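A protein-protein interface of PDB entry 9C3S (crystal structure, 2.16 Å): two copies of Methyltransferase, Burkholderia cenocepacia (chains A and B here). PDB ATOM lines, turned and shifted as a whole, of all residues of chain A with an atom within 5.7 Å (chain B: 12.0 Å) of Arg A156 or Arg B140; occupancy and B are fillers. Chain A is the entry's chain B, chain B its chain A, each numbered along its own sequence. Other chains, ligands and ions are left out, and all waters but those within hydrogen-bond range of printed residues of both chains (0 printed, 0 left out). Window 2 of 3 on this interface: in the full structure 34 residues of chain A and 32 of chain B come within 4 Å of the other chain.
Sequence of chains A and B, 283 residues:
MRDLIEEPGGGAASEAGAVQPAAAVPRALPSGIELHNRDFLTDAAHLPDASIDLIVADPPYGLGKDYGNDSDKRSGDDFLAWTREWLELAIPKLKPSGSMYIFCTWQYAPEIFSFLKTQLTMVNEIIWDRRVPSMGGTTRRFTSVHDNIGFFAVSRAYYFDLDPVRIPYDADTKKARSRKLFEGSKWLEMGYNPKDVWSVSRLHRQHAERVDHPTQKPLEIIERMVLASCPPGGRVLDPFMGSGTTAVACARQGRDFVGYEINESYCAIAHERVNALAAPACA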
ATOM      1  N   VAL A 123      -1.102 -12.710   0.229  1.00  0.00           N
ATOM      2  CA  VAL A 123      -1.506 -13.914   0.946  1.00  0.00           C
ATOM      3  C   VAL A 123      -0.462 -14.310   1.978  1.00  0.00           C
ATOM      4  O   VAL A 123      -0.806 -14.717   3.092  1.00  0.00           O
ATOM      5  CB  VAL A 123      -1.768 -15.061  -0.048  1.00  0.00           C
ATOM      6  CG1 VAL A 123      -1.987 -16.358   0.704  1.00  0.00           C
ATOM      7  CG2 VAL A 123      -2.962 -14.738  -0.923  1.00  0.00           C
ATOM      8  N   PHE A 151       4.001 -13.236  -1.565  1.00  0.00           N
ATOM      9  CA  PHE A 151       3.090 -14.188  -2.191  1.00  0.00           C
ATOM     10  C   PHE A 151       1.741 -13.484  -2.278  1.00  0.00           C
ATOM     11  O   PHE A 151       1.028 -13.376  -1.270  1.00  0.00           O
ATOM     12  CB  PHE A 151       3.018 -15.485  -1.381  1.00  0.00           C
ATOM     13  CG  PHE A 151       2.003 -16.479  -1.889  1.00  0.00           C
ATOM     14  CD1 PHE A 151       1.749 -16.615  -3.242  1.00  0.00           C
ATOM     15  CD2 PHE A 151       1.315 -17.292  -1.003  1.00  0.00           C
ATOM     16  CE1 PHE A 151       0.819 -17.535  -3.698  1.00  0.00           C
ATOM     17  CE2 PHE A 151       0.387 -18.210  -1.453  1.00  0.00           C
ATOM     18  CZ  PHE A 151       0.139 -18.333  -2.800  1.00  0.00           C
ATOM     19  N   VAL A 154      -4.351 -12.263  -7.373  1.00  0.00           N
ATOM     20  CA  VAL A 154      -5.239 -11.312  -8.041  1.00  0.00           C
ATOM     21  C   VAL A 154      -6.562 -11.219  -7.296  1.00  0.00           C
ATOM     22  O   VAL A 154      -6.982 -10.138  -6.864  1.00  0.00           O
ATOM     23  CB  VAL A 154      -5.465 -11.717  -9.509  1.00  0.00           C
ATOM     24  CG1 VAL A 154      -6.536 -10.834 -10.130  1.00  0.00           C
ATOM     25  CG2 VAL A 154      -4.170 -11.638 -10.301  1.00  0.00           C
ATOM     26  N   SER A 155      -7.232 -12.352  -7.135  1.00  0.00           N
ATOM     27  CA  SER A 155      -8.549 -12.436  -6.525  1.00  0.00           C
ATOM     28  C   SER A 155      -8.502 -13.408  -5.351  1.00  0.00           C
ATOM     29  O   SER A 155      -7.470 -14.013  -5.051  1.00  0.00           O
ATOM     30  CB  SER A 155      -9.593 -12.872  -7.555  1.00  0.00           C
ATOM     31  OG  SER A 155     -10.674 -13.542  -6.932  1.00  0.00           O
ATOM     32  N   ARG A 156      -9.646 -13.560  -4.690  1.00  0.00           N
ATOM     33  CA  ARG A 156      -9.742 -14.431  -3.527  1.00  0.00           C
ATOM     34  C   ARG A 156      -9.908 -15.896  -3.901  1.00  0.00           C
ATOM     35  O   ARG A 156      -9.775 -16.759  -3.026  1.00  0.00           O
ATOM     36  CB  ARG A 156     -10.914 -13.997  -2.645  1.00  0.00           C
ATOM     37  CG  ARG A 156     -10.959 -12.501  -2.358  1.00  0.00           C
ATOM     38  CD  ARG A 156     -12.376 -12.042  -2.086  1.00  0.00           C
ATOM     39  NE  ARG A 156     -12.834 -12.477  -0.773  1.00  0.00           N
ATOM     40  CZ  ARG A 156     -13.959 -12.076  -0.199  1.00  0.00           C
ATOM     41  NH1 ARG A 156     -14.783 -11.235  -0.805  1.00  0.00           N
ATOM     42  NH2 ARG A 156     -14.266 -12.528   1.013  1.00  0.00           N
ATOM     43  N   ALA A 157     -10.195 -16.194  -5.169  1.00  0.00           N
ATOM     44  CA  ALA A 157     -10.316 -17.563  -5.651  1.00  0.00           C
ATOM     45  C   ALA A 157      -9.015 -18.067  -6.266  1.00  0.00           C
ATOM     46  O   ALA A 157      -9.038 -18.933  -7.147  1.00  0.00           O
ATOM     47  CB  ALA A 157     -11.456 -17.666  -6.662  1.00  0.00           C
ATOM     48  N   TYR A 158      -7.879 -17.536  -5.820  1.00  0.00           N
ATOM     49  CA  TYR A 158      -6.600 -17.956  -6.372  1.00  0.00           C
ATOM     50  C   TYR A 158      -6.415 -19.456  -6.198  1.00  0.00           C
ATOM     51  O   TYR A 158      -6.884 -20.060  -5.230  1.00  0.00           O
ATOM     52  CB  TYR A 158      -5.443 -17.213  -5.700  1.00  0.00           C
ATOM     53  CG  TYR A 158      -5.333 -17.440  -4.204  1.00  0.00           C
ATOM     54  CD1 TYR A 158      -6.115 -16.717  -3.315  1.00  0.00           C
ATOM     55  CD2 TYR A 158      -4.447 -18.376  -3.684  1.00  0.00           C
ATOM     56  CE1 TYR A 158      -6.018 -16.915  -1.949  1.00  0.00           C
ATOM     57  CE2 TYR A 158      -4.345 -18.583  -2.316  1.00  0.00           C
ATOM     58  CZ  TYR A 158      -5.134 -17.847  -1.456  1.00  0.00           C
ATOM     59  OH  TYR A 158      -5.049 -18.041  -0.095  1.00  0.00           O
ATOM     60  N   TYR A 159      -5.725 -20.061  -7.159  1.00  0.00           N
ATOM     61  CA  TYR A 159      -5.413 -21.476  -7.064  1.00  0.00           C
ATOM     62  C   TYR A 159      -4.319 -21.703  -6.028  1.00  0.00           C
ATOM     63  O   TYR A 159      -3.342 -20.950  -5.956  1.00  0.00           O
ATOM     64  CB  TYR A 159      -4.975 -22.016  -8.424  1.00  0.00           C
ATOM     65  CG  TYR A 159      -4.356 -23.386  -8.346  1.00  0.00           C
ATOM     66  CD1 TYR A 159      -5.149 -24.526  -8.305  1.00  0.00           C
ATOM     67  CD2 TYR A 159      -2.979 -23.542  -8.298  1.00  0.00           C
ATOM     68  CE1 TYR A 159      -4.585 -25.786  -8.227  1.00  0.00           C
ATOM     69  CE2 TYR A 159      -2.404 -24.796  -8.217  1.00  0.00           C
ATOM     70  CZ  TYR A 159      -3.211 -25.914  -8.183  1.00  0.00           C
ATOM     71  OH  TYR A 159      -2.637 -27.163  -8.103  1.00  0.00           O
ATOM     72  N   PHE A 160      -4.493 -22.746  -5.218  1.00  0.00           N
ATOM     73  CA  PHE A 160      -3.500 -23.108  -4.209  1.00  0.00           C
ATOM     74  C   PHE A 160      -3.762 -24.538  -3.778  1.00  0.00           C
ATOM     75  O   PHE A 160      -4.851 -24.840  -3.277  1.00  0.00           O
ATOM     76  CB  PHE A 160      -3.560 -22.169  -3.008  1.00  0.00           C
ATOM     77  CG  PHE A 160      -2.523 -22.466  -1.960  1.00  0.00           C
ATOM     78  CD1 PHE A 160      -1.240 -21.960  -2.072  1.00  0.00           C
ATOM     79  CD2 PHE A 160      -2.831 -23.258  -0.869  1.00  0.00           C
ATOM     80  CE1 PHE A 160      -0.287 -22.237  -1.113  1.00  0.00           C
ATOM     81  CE2 PHE A 160      -1.882 -23.536   0.094  1.00  0.00           C
ATOM     82  CZ  PHE A 160      -0.608 -23.027  -0.028  1.00  0.00           C
ATOM     83  N   TRP B 106       3.729  -9.412   9.401  1.00  0.00           N
ATOM     84  CA  TRP B 106       3.929  -9.222   7.949  1.00  0.00           C
ATOM     85  C   TRP B 106       2.728  -8.512   7.351  1.00  0.00           C
ATOM     86  O   TRP B 106       2.888  -7.850   6.327  1.00  0.00           O
ATOM     87  CB  TRP B 106       4.112 -10.599   7.311  1.00  0.00           C
ATOM     88  CG  TRP B 106       2.866 -11.437   7.287  1.00  0.00           C
ATOM     89  CD1 TRP B 106       2.417 -12.278   8.260  1.00  0.00           C
ATOM     90  CD2 TRP B 106       1.901 -11.499   6.222  1.00  0.00           C
ATOM     91  NE1 TRP B 106       1.245 -12.863   7.873  1.00  0.00           N
ATOM     92  CE2 TRP B 106       0.902 -12.404   6.630  1.00  0.00           C
ATOM     93  CE3 TRP B 106       1.788 -10.883   4.974  1.00  0.00           C
ATOM     94  CZ2 TRP B 106      -0.194 -12.706   5.829  1.00  0.00           C
ATOM     95  CZ3 TRP B 106       0.703 -11.185   4.186  1.00  0.00           C
ATOM     96  CH2 TRP B 106      -0.274 -12.080   4.609  1.00  0.00           C
ATOM     97  N   SER B 134       1.264 -20.744  13.980  1.00  0.00           N
ATOM     98  CA  SER B 134      -0.061 -20.404  14.471  1.00  0.00           C
ATOM     99  C   SER B 134      -1.074 -21.456  14.041  1.00  0.00           C
ATOM    100  O   SER B 134      -0.978 -22.044  12.959  1.00  0.00           O
ATOM    101  CB  SER B 134      -0.487 -19.031  13.965  1.00  0.00           C
ATOM    102  OG  SER B 134       0.218 -18.005  14.645  1.00  0.00           O
ATOM    103  N   MET B 135      -2.052 -21.696  14.911  1.00  0.00           N
ATOM    104  CA  MET B 135      -3.062 -22.710  14.666  1.00  0.00           C
ATOM    105  C   MET B 135      -4.254 -22.060  13.964  1.00  0.00           C
ATOM    106  O   MET B 135      -4.249 -20.865  13.662  1.00  0.00           O
ATOM    107  CB  MET B 135      -3.463 -23.373  15.987  1.00  0.00           C
ATOM    108  CG  MET B 135      -2.750 -24.699  16.304  1.00  0.00           C
ATOM    109  SD  MET B 135      -2.562 -25.852  14.927  1.00  0.00           S
ATOM    110  CE  MET B 135      -0.797 -25.825  14.693  1.00  0.00           C
ATOM    111  N   GLY B 136      -5.285 -22.853  13.689  1.00  0.00           N
ATOM    112  CA  GLY B 136      -6.436 -22.343  12.968  1.00  0.00           C
ATOM    113  C   GLY B 136      -7.146 -23.391  12.137  1.00  0.00           C
ATOM    114  O   GLY B 136      -8.336 -23.645  12.345  1.00  0.00           O
ATOM    115  N   GLY B 137      -6.433 -23.996  11.189  1.00  0.00           N
ATOM    116  CA  GLY B 137      -7.018 -25.026  10.350  1.00  0.00           C
ATOM    117  C   GLY B 137      -6.913 -24.735   8.867  1.00  0.00           C
ATOM    118  O   GLY B 137      -7.536 -25.423   8.052  1.00  0.00           O
ATOM    119  N   THR B 138      -6.132 -23.724   8.495  1.00  0.00           N
ATOM    120  CA  THR B 138      -6.098 -23.309   7.103  1.00  0.00           C
ATOM    121  C   THR B 138      -5.416 -24.357   6.229  1.00  0.00           C
ATOM    122  O   THR B 138      -4.666 -25.220   6.694  1.00  0.00           O
ATOM    123  CB  THR B 138      -5.376 -21.970   6.942  1.00  0.00           C
ATOM    124  OG1 THR B 138      -5.496 -21.529   5.584  1.00  0.00           O
ATOM    125  CG2 THR B 138      -3.897 -22.096   7.299  1.00  0.00           C
ATOM    126  N   THR B 139      -5.704 -24.261   4.936  1.00  0.00           N
ATOM    127  CA  THR B 139      -5.082 -25.082   3.910  1.00  0.00           C
ATOM    128  C   THR B 139      -4.724 -24.243   2.692  1.00  0.00           C
ATOM    129  O   THR B 139      -4.071 -24.753   1.775  1.00  0.00           O
ATOM    130  CB  THR B 139      -6.035 -26.236   3.519  1.00  0.00           C
ATOM    131  OG1 THR B 139      -5.913 -27.299   4.473  1.00  0.00           O
ATOM    132  CG2 THR B 139      -5.758 -26.785   2.114  1.00  0.00           C
ATOM    133  N   ARG B 140      -5.088 -22.962   2.679  1.00  0.00           N
ATOM    134  CA  ARG B 140      -5.044 -22.131   1.488  1.00  0.00           C
ATOM    135  C   ARG B 140      -3.952 -21.069   1.566  1.00  0.00           C
ATOM    136  O   ARG B 140      -4.047 -20.022   0.922  1.00  0.00           O
ATOM    137  CB  ARG B 140      -6.411 -21.489   1.264  1.00  0.00           C
ATOM    138  CG  ARG B 140      -7.396 -22.444   0.612  1.00  0.00           C
ATOM    139  CD  ARG B 140      -8.679 -21.759   0.184  1.00  0.00           C
ATOM    140  NE  ARG B 140      -8.461 -20.574  -0.638  1.00  0.00           N
ATOM    141  CZ  ARG B 140      -7.901 -20.575  -1.842  1.00  0.00           C
ATOM    142  NH1 ARG B 140      -7.458 -21.689  -2.402  1.00  0.00           N
ATOM    143  NH2 ARG B 140      -7.782 -19.426  -2.500  1.00  0.00           N
ATOM    144  N   ARG B 141      -2.904 -21.333   2.342  1.00  0.00           N
ATOM    145  CA  ARG B 141      -1.772 -20.423   2.465  1.00  0.00           C
ATOM    146  C   ARG B 141      -0.758 -21.080   3.391  1.00  0.00           C
ATOM    147  O   ARG B 141      -1.057 -22.061   4.079  1.00  0.00           O
ATOM    148  CB  ARG B 141      -2.177 -19.045   3.003  1.00  0.00           C
ATOM    149  CG  ARG B 141      -1.964 -18.872   4.507  1.00  0.00           C
ATOM    150  CD  ARG B 141      -2.877 -17.811   5.096  1.00  0.00           C
ATOM    151  NE  ARG B 141      -2.864 -16.565   4.340  1.00  0.00           N
ATOM    152  CZ  ARG B 141      -3.894 -15.733   4.244  1.00  0.00           C
ATOM    153  NH1 ARG B 141      -5.051 -15.989   4.833  1.00  0.00           N
ATOM    154  NH2 ARG B 141      -3.759 -14.616   3.537  1.00  0.00           N
ATOM    155  N   PHE B 142       0.445 -20.516   3.409  1.00  0.00           N
ATOM    156  CA  PHE B 142       1.487 -21.002   4.296  1.00  0.00           C
ATOM    157  C   PHE B 142       1.269 -20.456   5.700  1.00  0.00           C
ATOM    158  O   PHE B 142       0.896 -19.294   5.884  1.00  0.00           O
ATOM    159  CB  PHE B 142       2.858 -20.606   3.755  1.00  0.00           C
ATOM    160  CG  PHE B 142       3.155 -21.200   2.408  1.00  0.00           C
ATOM    161  CD1 PHE B 142       3.390 -22.556   2.274  1.00  0.00           C
ATOM    162  CD2 PHE B 142       3.171 -20.411   1.274  1.00  0.00           C
ATOM    163  CE1 PHE B 142       3.652 -23.113   1.037  1.00  0.00           C
ATOM    164  CE2 PHE B 142       3.431 -20.964   0.032  1.00  0.00           C
ATOM    165  CZ  PHE B 142       3.674 -22.317  -0.084  1.00  0.00           C
ATOM    166  N   THR B 143       1.497 -21.309   6.690  1.00  0.00           N
ATOM    167  CA  THR B 143       1.146 -21.000   8.066  1.00  0.00           C
ATOM    168  C   THR B 143       2.136 -20.009   8.674  1.00  0.00           C
ATOM    169  O   THR B 143       3.323 -19.995   8.335  1.00  0.00           O
ATOM    170  CB  THR B 143       1.105 -22.288   8.888  1.00  0.00           C
ATOM    171  OG1 THR B 143       2.093 -23.198   8.390  1.00  0.00           O
ATOM    172  CG2 THR B 143      -0.267 -22.943   8.776  1.00  0.00           C
ATOM    173  N   SER B 144       1.631 -19.173   9.581  1.00  0.00           N
ATOM    174  CA  SER B 144       2.444 -18.127  10.192  1.00  0.00           C
ATOM    175  C   SER B 144       3.369 -18.722  11.241  1.00  0.00           C
ATOM    176  O   SER B 144       2.919 -19.434  12.143  1.00  0.00           O
ATOM    177  CB  SER B 144       1.559 -17.059  10.832  1.00  0.00           C
ATOM    178  OG  SER B 144       2.352 -16.074  11.483  1.00  0.00           O
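Printed residues of chain A that touch a printed residue of chain B: Val A123, Arg A156, Tyr A158 and Phe A160.
Of the 12 printed residues of chain B, 4 touch a printed residue of chain A.
Hydrophobic or aromatic side chains of chain B that line the printed part of chain A: Trp B106.
Among the printed residues, no Asp or Glu carboxylate lies within 4 Å of a Lys or Arg side-chain nitrogen of the other chain.
No position is printed for both chains.
The side-chain hydroxyl (OG1) of Thr B138 sits at hydrogen-bond distance from the backbone NH (N) of Arg B140.
The backbone NH (N) of Val A123 lies within hydrogen-bond range of the backbone carbonyl oxygen (O) of Phe A151 (2.7 Å).
Val A123 touches two residues of chain B.
No residue of chain B comes within 4 Å of Ser A155.
Of chain B, only Arg B140 (3.4 Å) comes within 4 Å of Arg A156.
Tyr A158 touches just one residue of chain B: Arg B140.
Phe A160 touches just these residues of chain B: Thr B139, Arg B140 and Arg B141.
Of the printed residues of chain A, Trp B106 touches Val A123.
Thr B138 touches none of the printed residues of chain A.
Of the printed residues of chain A, Thr B139 touches Phe A160 (3.0 Å).
Printed residues of chain A within 4 Å of Arg B140: Arg A156, Tyr A158 and Phe A160.
Printed residues of chain A within 4 Å of Arg B141: Val A123 (3.0 Å) and Phe A160 (3.3 Å).
O of Arg A156 is in hydrogen-bond range of NH2 of Arg B140 (3.4 Å).
The side-chain hydroxyl of Tyr A158 lies within hydrogen-bond range of the backbone carbonyl oxygen of Arg B140 (2.4 Å).
NH2 of Arg B141 lies within hydrogen-bond range of O of Val A123, 3.0 Å away.
Among the printed residues, merely in contact across the chains: Phe A160 with Thr B139, Val A123 with Trp B106, Phe A160 with Arg B141 and Phe A160 with Arg B140.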
